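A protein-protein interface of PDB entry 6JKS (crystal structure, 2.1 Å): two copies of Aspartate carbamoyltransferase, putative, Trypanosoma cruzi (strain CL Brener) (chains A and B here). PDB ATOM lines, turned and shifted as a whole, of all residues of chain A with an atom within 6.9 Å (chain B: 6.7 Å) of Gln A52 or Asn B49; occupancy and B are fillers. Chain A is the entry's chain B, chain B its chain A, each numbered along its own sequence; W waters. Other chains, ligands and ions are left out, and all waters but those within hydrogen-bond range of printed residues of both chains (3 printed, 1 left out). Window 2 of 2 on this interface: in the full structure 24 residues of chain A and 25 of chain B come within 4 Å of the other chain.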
ATOM      1  N   LEU A  48     -16.923   4.093  -9.825  1.00  0.00           N
ATOM      2  CA  LEU A  48     -15.709   3.254  -9.822  1.00  0.00           C
ATOM      3  C   LEU A  48     -14.813   3.623 -10.988  1.00  0.00           C
ATOM      4  O   LEU A  48     -15.296   3.785 -12.106  1.00  0.00           O
ATOM      5  CB  LEU A  48     -16.070   1.753  -9.857  1.00  0.00           C
ATOM      6  CG  LEU A  48     -16.975   1.250  -8.739  1.00  0.00           C
ATOM      7  CD1 LEU A  48     -17.204  -0.273  -8.798  1.00  0.00           C
ATOM      8  CD2 LEU A  48     -16.380   1.654  -7.362  1.00  0.00           C
ATOM      9  N   ASN A  49     -13.514   3.768 -10.730  1.00  0.00           N
ATOM     10  CA  ASN A  49     -12.558   4.139 -11.776  1.00  0.00           C
ATOM     11  C   ASN A  49     -11.501   3.088 -12.094  1.00  0.00           C
ATOM     12  O   ASN A  49     -10.486   3.395 -12.740  1.00  0.00           O
ATOM     13  CB  ASN A  49     -11.833   5.425 -11.387  1.00  0.00           C
ATOM     14  CG  ASN A  49     -11.874   6.440 -12.468  1.00  0.00           C
ATOM     15  OD1 ASN A  49     -12.948   6.899 -12.844  1.00  0.00           O
ATOM     16  ND2 ASN A  49     -10.699   6.834 -12.975  1.00  0.00           N
ATOM     17  N   LEU A  50     -11.766   1.852 -11.702  1.00  0.00           N
ATOM     18  CA  LEU A  50     -10.803   0.754 -11.743  1.00  0.00           C
ATOM     19  C   LEU A  50     -10.231   0.376 -13.099  1.00  0.00           C
ATOM     20  O   LEU A  50      -9.082  -0.050 -13.158  1.00  0.00           O
ATOM     21  CB  LEU A  50     -11.408  -0.498 -11.085  1.00  0.00           C
ATOM     22  CG  LEU A  50     -11.910  -0.355  -9.641  1.00  0.00           C
ATOM     23  CD1 LEU A  50     -12.724  -1.594  -9.203  1.00  0.00           C
ATOM     24  CD2 LEU A  50     -10.768  -0.079  -8.629  1.00  0.00           C
ATOM     25  N   LEU A  51     -11.019   0.504 -14.181  1.00  0.00           N
ATOM     26  CA  LEU A  51     -10.562   0.063 -15.511  1.00  0.00           C
ATOM     27  C   LEU A  51     -10.531   1.162 -16.569  1.00  0.00           C
ATOM     28  O   LEU A  51     -10.719   0.906 -17.756  1.00  0.00           O
ATOM     29  CB  LEU A  51     -11.373  -1.152 -16.005  1.00  0.00           C
ATOM     30  CG  LEU A  51     -11.197  -2.445 -15.183  1.00  0.00           C
ATOM     31  CD1 LEU A  51     -12.089  -3.524 -15.716  1.00  0.00           C
ATOM     32  CD2 LEU A  51      -9.768  -2.939 -15.178  1.00  0.00           C
ATOM     33  N   GLN A  52     -10.269   2.391 -16.137  1.00  0.00           N
ATOM     34  CA  GLN A  52     -10.116   3.505 -17.066  1.00  0.00           C
ATOM     35  C   GLN A  52      -9.016   3.172 -18.038  1.00  0.00           C
ATOM     36  O   GLN A  52      -7.990   2.626 -17.640  1.00  0.00           O
ATOM     37  CB  GLN A  52      -9.819   4.834 -16.342  1.00  0.00           C
ATOM     38  CG  GLN A  52     -10.013   6.073 -17.273  1.00  0.00           C
ATOM     39  CD  GLN A  52      -9.550   7.409 -16.630  1.00  0.00           C
ATOM     40  OE1 GLN A  52      -9.445   7.513 -15.407  1.00  0.00           O
ATOM     41  NE2 GLN A  52      -9.273   8.413 -17.460  1.00  0.00           N
ATOM     42  N   GLY A  53      -9.247   3.479 -19.316  1.00  0.00           N
ATOM     43  CA  GLY A  53      -8.282   3.161 -20.353  1.00  0.00           C
ATOM     44  C   GLY A  53      -8.251   1.727 -20.847  1.00  0.00           C
ATOM     45  O   GLY A  53      -7.425   1.385 -21.713  1.00  0.00           O
ATOM     46  N   ARG A  54      -9.109   0.858 -20.320  1.00  0.00           N
ATOM     47  CA  ARG A  54      -9.139  -0.538 -20.826  1.00  0.00           C
ATOM     48  C   ARG A  54     -10.363  -0.750 -21.690  1.00  0.00           C
ATOM     49  O   ARG A  54     -11.430  -0.141 -21.466  1.00  0.00           O
ATOM     50  CB  ARG A  54      -9.103  -1.575 -19.702  1.00  0.00           C
ATOM     51  CG  ARG A  54      -8.002  -1.351 -18.622  1.00  0.00           C
ATOM     52  CD  ARG A  54      -6.548  -1.524 -19.106  1.00  0.00           C
ATOM     53  NE  ARG A  54      -5.635  -0.888 -18.138  1.00  0.00           N
ATOM     54  CZ  ARG A  54      -4.686   0.023 -18.405  1.00  0.00           C
ATOM     55  NH1 ARG A  54      -4.408   0.416 -19.658  1.00  0.00           N
ATOM     56  NH2 ARG A  54      -3.954   0.507 -17.392  1.00  0.00           N
ATOM     57  N   ILE A  55     -10.221  -1.627 -22.683  1.00  0.00           N
ATOM     58  CA  ILE A  55     -11.259  -1.767 -23.689  1.00  0.00           C
ATOM     59  C   ILE A  55     -11.793  -3.191 -23.721  1.00  0.00           C
ATOM     60  O   ILE A  55     -11.037  -4.144 -23.868  1.00  0.00           O
ATOM     61  CB  ILE A  55     -10.737  -1.382 -25.092  1.00  0.00           C
ATOM     62  CG1 ILE A  55     -10.380   0.117 -25.142  1.00  0.00           C
ATOM     63  CG2 ILE A  55     -11.726  -1.796 -26.141  1.00  0.00           C
ATOM     64  CD1 ILE A  55      -9.946   0.605 -26.539  1.00  0.00           C
ATOM     65  N   LEU A  78     -17.248  -0.100 -14.263  1.00  0.00           N
ATOM     66  CA  LEU A  78     -15.903  -0.254 -13.728  1.00  0.00           C
ATOM     67  C   LEU A  78     -15.009   0.900 -14.193  1.00  0.00           C
ATOM     68  O   LEU A  78     -13.843   0.937 -13.832  1.00  0.00           O
ATOM     69  CB  LEU A  78     -15.288  -1.612 -14.131  1.00  0.00           C
ATOM     70  CG  LEU A  78     -15.846  -2.841 -13.384  1.00  0.00           C
ATOM     71  CD1 LEU A  78     -15.410  -4.195 -14.064  1.00  0.00           C
ATOM     72  CD2 LEU A  78     -15.496  -2.856 -11.901  1.00  0.00           C
ATOM     73  N   GLY A  79     -15.540   1.801 -15.026  1.00  0.00           N
ATOM     74  CA  GLY A  79     -14.732   2.869 -15.602  1.00  0.00           C
ATOM     75  C   GLY A  79     -14.034   2.543 -16.915  1.00  0.00           C
ATOM     76  O   GLY A  79     -13.280   3.361 -17.433  1.00  0.00           O
ATOM     77  N   GLY A  80     -14.294   1.351 -17.456  1.00  0.00           N
ATOM     78  CA  GLY A  80     -13.710   0.915 -18.724  1.00  0.00           C
ATOM     79  C   GLY A  80     -14.556   1.299 -19.918  1.00  0.00           C
ATOM     80  O   GLY A  80     -15.614   1.919 -19.769  1.00  0.00           O
ATOM     81  N   SER A  81     -14.110   0.892 -21.107  1.00  0.00           N
ATOM     82  CA  SER A  81     -14.762   1.327 -22.326  1.00  0.00           C
ATOM     83  C   SER A  81     -15.086   0.149 -23.236  1.00  0.00           C
ATOM     84  O   SER A  81     -14.569  -0.951 -23.054  1.00  0.00           O
ATOM     85  CB  SER A  81     -13.873   2.321 -23.061  1.00  0.00           C
ATOM     86  OG  SER A  81     -13.642   3.458 -22.259  1.00  0.00           O
ATOM     87  N   GLY B  45       1.029   0.670 -19.862  1.00  0.00           N
ATOM     88  CA  GLY B  45      -0.200   0.739 -19.056  1.00  0.00           C
ATOM     89  C   GLY B  45      -0.646   2.133 -18.633  1.00  0.00           C
ATOM     90  O   GLY B  45      -1.572   2.271 -17.833  1.00  0.00           O
ATOM     91  N   VAL B  47      -2.556   5.644 -18.658  1.00  0.00           N
ATOM     92  CA  VAL B  47      -3.868   6.061 -19.083  1.00  0.00           C
ATOM     93  C   VAL B  47      -3.817   7.515 -19.575  1.00  0.00           C
ATOM     94  O   VAL B  47      -3.389   8.404 -18.849  1.00  0.00           O
ATOM     95  CB  VAL B  47      -4.865   5.921 -17.922  1.00  0.00           C
ATOM     96  CG1 VAL B  47      -6.236   6.436 -18.335  1.00  0.00           C
ATOM     97  CG2 VAL B  47      -4.957   4.444 -17.488  1.00  0.00           C
ATOM     98  N   LEU B  48      -4.252   7.764 -20.807  1.00  0.00           N
ATOM     99  CA  LEU B  48      -4.219   9.142 -21.336  1.00  0.00           C
ATOM    100  C   LEU B  48      -5.579   9.829 -21.246  1.00  0.00           C
ATOM    101  O   LEU B  48      -6.619   9.201 -21.514  1.00  0.00           O
ATOM    102  CB  LEU B  48      -3.673   9.176 -22.771  1.00  0.00           C
ATOM    103  CG  LEU B  48      -2.389   8.368 -23.045  1.00  0.00           C
ATOM    104  CD1 LEU B  48      -2.105   8.311 -24.545  1.00  0.00           C
ATOM    105  CD2 LEU B  48      -1.165   8.890 -22.280  1.00  0.00           C
ATOM    106  N   ASN B  49      -5.575  11.110 -20.880  1.00  0.00           N
ATOM    107  CA  ASN B  49      -6.817  11.888 -20.771  1.00  0.00           C
ATOM    108  C   ASN B  49      -6.883  13.166 -21.646  1.00  0.00           C
ATOM    109  O   ASN B  49      -7.671  14.104 -21.384  1.00  0.00           O
ATOM    110  CB  ASN B  49      -7.185  12.150 -19.301  1.00  0.00           C
ATOM    111  CG  ASN B  49      -8.673  11.972 -19.045  1.00  0.00           C
ATOM    112  OD1 ASN B  49      -9.503  12.280 -19.903  1.00  0.00           O
ATOM    113  ND2 ASN B  49      -9.020  11.452 -17.878  1.00  0.00           N
ATOM    114  N   LEU B  50      -6.111  13.139 -22.721  1.00  0.00           N
ATOM    115  CA  LEU B  50      -5.921  14.226 -23.662  1.00  0.00           C
ATOM    116  C   LEU B  50      -7.180  14.720 -24.397  1.00  0.00           C
ATOM    117  O   LEU B  50      -7.293  15.904 -24.661  1.00  0.00           O
ATOM    118  CB  LEU B  50      -4.887  13.783 -24.702  1.00  0.00           C
ATOM    119  CG  LEU B  50      -3.432  13.576 -24.242  1.00  0.00           C
ATOM    120  CD1 LEU B  50      -2.597  13.198 -25.442  1.00  0.00           C
ATOM    121  CD2 LEU B  50      -2.863  14.849 -23.568  1.00  0.00           C
ATOM    122  N   LEU B  51      -8.120  13.824 -24.735  1.00  0.00           N
ATOM    123  CA  LEU B  51      -9.327  14.261 -25.445  1.00  0.00           C
ATOM    124  C   LEU B  51     -10.619  14.023 -24.648  1.00  0.00           C
ATOM    125  O   LEU B  51     -11.689  13.790 -25.231  1.00  0.00           O
ATOM    126  CB  LEU B  51      -9.404  13.597 -26.841  1.00  0.00           C
ATOM    127  CG  LEU B  51      -8.305  13.943 -27.860  1.00  0.00           C
ATOM    128  CD1 LEU B  51      -8.529  13.172 -29.143  1.00  0.00           C
ATOM    129  CD2 LEU B  51      -8.253  15.455 -28.125  1.00  0.00           C
ATOM    130  N   GLN B  52     -10.525  14.042 -23.319  1.00  0.00           N
ATOM    131  CA  GLN B  52     -11.719  13.953 -22.494  1.00  0.00           C
ATOM    132  C   GLN B  52     -12.720  14.993 -22.971  1.00  0.00           C
ATOM    133  O   GLN B  52     -12.350  16.150 -23.216  1.00  0.00           O
ATOM    134  CB  GLN B  52     -11.436  14.151 -21.007  1.00  0.00           C
ATOM    135  CG  GLN B  52     -12.632  13.654 -20.108  1.00  0.00           C
ATOM    136  CD  GLN B  52     -12.382  13.840 -18.592  1.00  0.00           C
ATOM    137  OE1 GLN B  52     -11.275  14.221 -18.164  1.00  0.00           O
ATOM    138  NE2 GLN B  52     -13.405  13.557 -17.782  1.00  0.00           N
ATOM    139  N   GLY B  53     -13.970  14.562 -23.128  1.00  0.00           N
ATOM    140  CA  GLY B  53     -15.078  15.445 -23.516  1.00  0.00           C
ATOM    141  C   GLY B  53     -15.193  15.719 -25.009  1.00  0.00           C
ATOM    142  O   GLY B  53     -16.089  16.468 -25.422  1.00  0.00           O
ATOM    143  N   ARG B  77      -8.573   5.469 -26.166  1.00  0.00           N
ATOM    144  CA  ARG B  77      -7.307   5.395 -25.472  1.00  0.00           C
ATOM    145  C   ARG B  77      -6.687   6.779 -25.289  1.00  0.00           C
ATOM    146  O   ARG B  77      -5.660   6.910 -24.594  1.00  0.00           O
ATOM    147  CB  ARG B  77      -6.325   4.451 -26.181  1.00  0.00           C
ATOM    148  CG  ARG B  77      -6.815   3.014 -26.161  1.00  0.00           C
ATOM    149  CD  ARG B  77      -5.720   2.028 -26.567  1.00  0.00           C
ATOM    150  NE  ARG B  77      -6.253   0.675 -26.461  1.00  0.00           N
ATOM    151  CZ  ARG B  77      -6.259  -0.055 -25.352  1.00  0.00           C
ATOM    152  NH1 ARG B  77      -5.742   0.434 -24.213  1.00  0.00           N
ATOM    153  NH2 ARG B  77      -6.769  -1.294 -25.387  1.00  0.00           N
ATOM    154  N   LEU B  78      -7.298   7.785 -25.935  1.00  0.00           N
ATOM    155  CA  LEU B  78      -6.891   9.186 -25.762  1.00  0.00           C
ATOM    156  C   LEU B  78      -7.792   9.863 -24.736  1.00  0.00           C
ATOM    157  O   LEU B  78      -7.607  11.060 -24.434  1.00  0.00           O
ATOM    158  CB  LEU B  78      -6.954   9.955 -27.097  1.00  0.00           C
ATOM    159  CG  LEU B  78      -5.882   9.628 -28.142  1.00  0.00           C
ATOM    160  CD1 LEU B  78      -6.261  10.287 -29.476  1.00  0.00           C
ATOM    161  CD2 LEU B  78      -4.456  10.059 -27.674  1.00  0.00           C
ATOM    162  N   GLY B  79      -8.772   9.101 -24.224  1.00  0.00           N
ATOM    163  CA  GLY B  79      -9.690   9.581 -23.209  1.00  0.00           C
ATOM    164  C   GLY B  79     -10.934  10.191 -23.833  1.00  0.00           C
ATOM    165  O   GLY B  79     -11.788  10.714 -23.112  1.00  0.00           O
ATOM    166  N   GLY B  80     -11.027  10.097 -25.163  1.00  0.00           N
ATOM    167  CA  GLY B  80     -12.159  10.621 -25.941  1.00  0.00           C
ATOM    168  C   GLY B  80     -13.335   9.652 -25.973  1.00  0.00           C
ATOM    169  O   GLY B  80     -13.280   8.553 -25.395  1.00  0.00           O
HETATM  170  O   HOH W   1      -4.610  -1.337 -22.157  1.00  0.00           O
HETATM  171  O   HOH W   2      -5.294   2.775 -22.673  1.00  0.00           O
HETATM  172  O   HOH W   3      -2.774   2.258 -21.076  1.00  0.00           O
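The backbone carbonyl oxygen (O) of Gly B45 lies within hydrogen-bond range of the guanidinium group (NH2) of Arg A54. The guanidinium group (NH1) of Arg B77 is in hydrogen-bond range of the backbone carbonyl oxygen (O) of Gly A53, 3.2 Å away. The side-chain amide nitrogen (ND2) of Asn B49 lies close to the side-chain amide nitrogen (NE2) of Gln A52 (3.1 Å).
The side-chain amide nitrogen (ND2) of Asn A49 lies within hydrogen-bond range of the side-chain amide oxygen (OE1) of Gln A52, 2.8 Å away. The side-chain amide oxygen (OD1) of Asn B49 lies close to the side-chain amide oxygen (OE1) of Gln B52 (3.2 Å). The backbone NH of Ser A81 lies within hydrogen-bond range of the backbone carbonyl oxygen of Arg A54 (2.9 Å). The backbone NH of Gln A52 lies close to the backbone carbonyl oxygen of Gly A79, 3.4 Å away.
Val B47 touches Gln A52 (CG2 to O, 3.5 Å). NE of Arg B77 touches CD1 of Ile A55, at 3.7 Å.
Asn A49 touches none of the printed residues of chain B. Leu A50 touches none of the printed residues of chain B. Of chain B, only Val B47 and Asn B49 come within 4 Å of Gln A52. Of the printed residues of chain B, Gly A53 touches Arg B77. Of the printed residues of chain B, Arg A54 touches Gly B45. Of the printed residues of chain B, Ile A55 touches Arg B77 (3.7 Å). Of the printed residues of chain A, Gly B45 touches Arg A54 (3.0 Å). Asn B49 touches just one residue of chain A: Gln A52 (3.1 Å). The nearest printed residue of chain A that does not touch Asn B49 is Asn A49 (6.9 Å). The nearest printed residue of chain A that does not touch Val B47 is Arg A54 (4.1 Å).
Of the 12 printed residues of chain A, 4 touch a printed residue of chain B. Hydrophobic or aromatic side chains of chain A within 4 Å of the printed part of chain B: Ile A55. Along chain A the printed residues that touch a printed residue of chain B span positions 52 to 55. Of the 12 printed residues of chain B, 4 touch a printed residue of chain A. Hydrophobic or aromatic side chains of chain B that line the printed part of chain A: Val B47. Among the printed residues, 5 pairs touch across the chains. Among the printed residues, no Asp or Glu carboxylate lies within 4 Å of a Lys or Arg side-chain nitrogen of the other chain.
Gln A52 touches Asn B49, but with the chains exchanged Asn A49 does not touch Gln B52 (8.3 Å).
Water W2 lies within hydrogen-bond range of the backbone carbonyl oxygen (O) of Gly A53 (2.7 Å) and the guanidinium group (NH1) of Arg B77 (2.8 Å). Water W3 lies within hydrogen-bond range of the guanidinium group (NH1) of Arg A54 and the backbone carbonyl oxygen (O) of Gly B45. Water W1 lies within hydrogen-bond range of the guanidinium group (NH1) of Arg B77 (2.9 Å) and the guanidinium group (NH1) of Arg A54 (3.1 Å).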
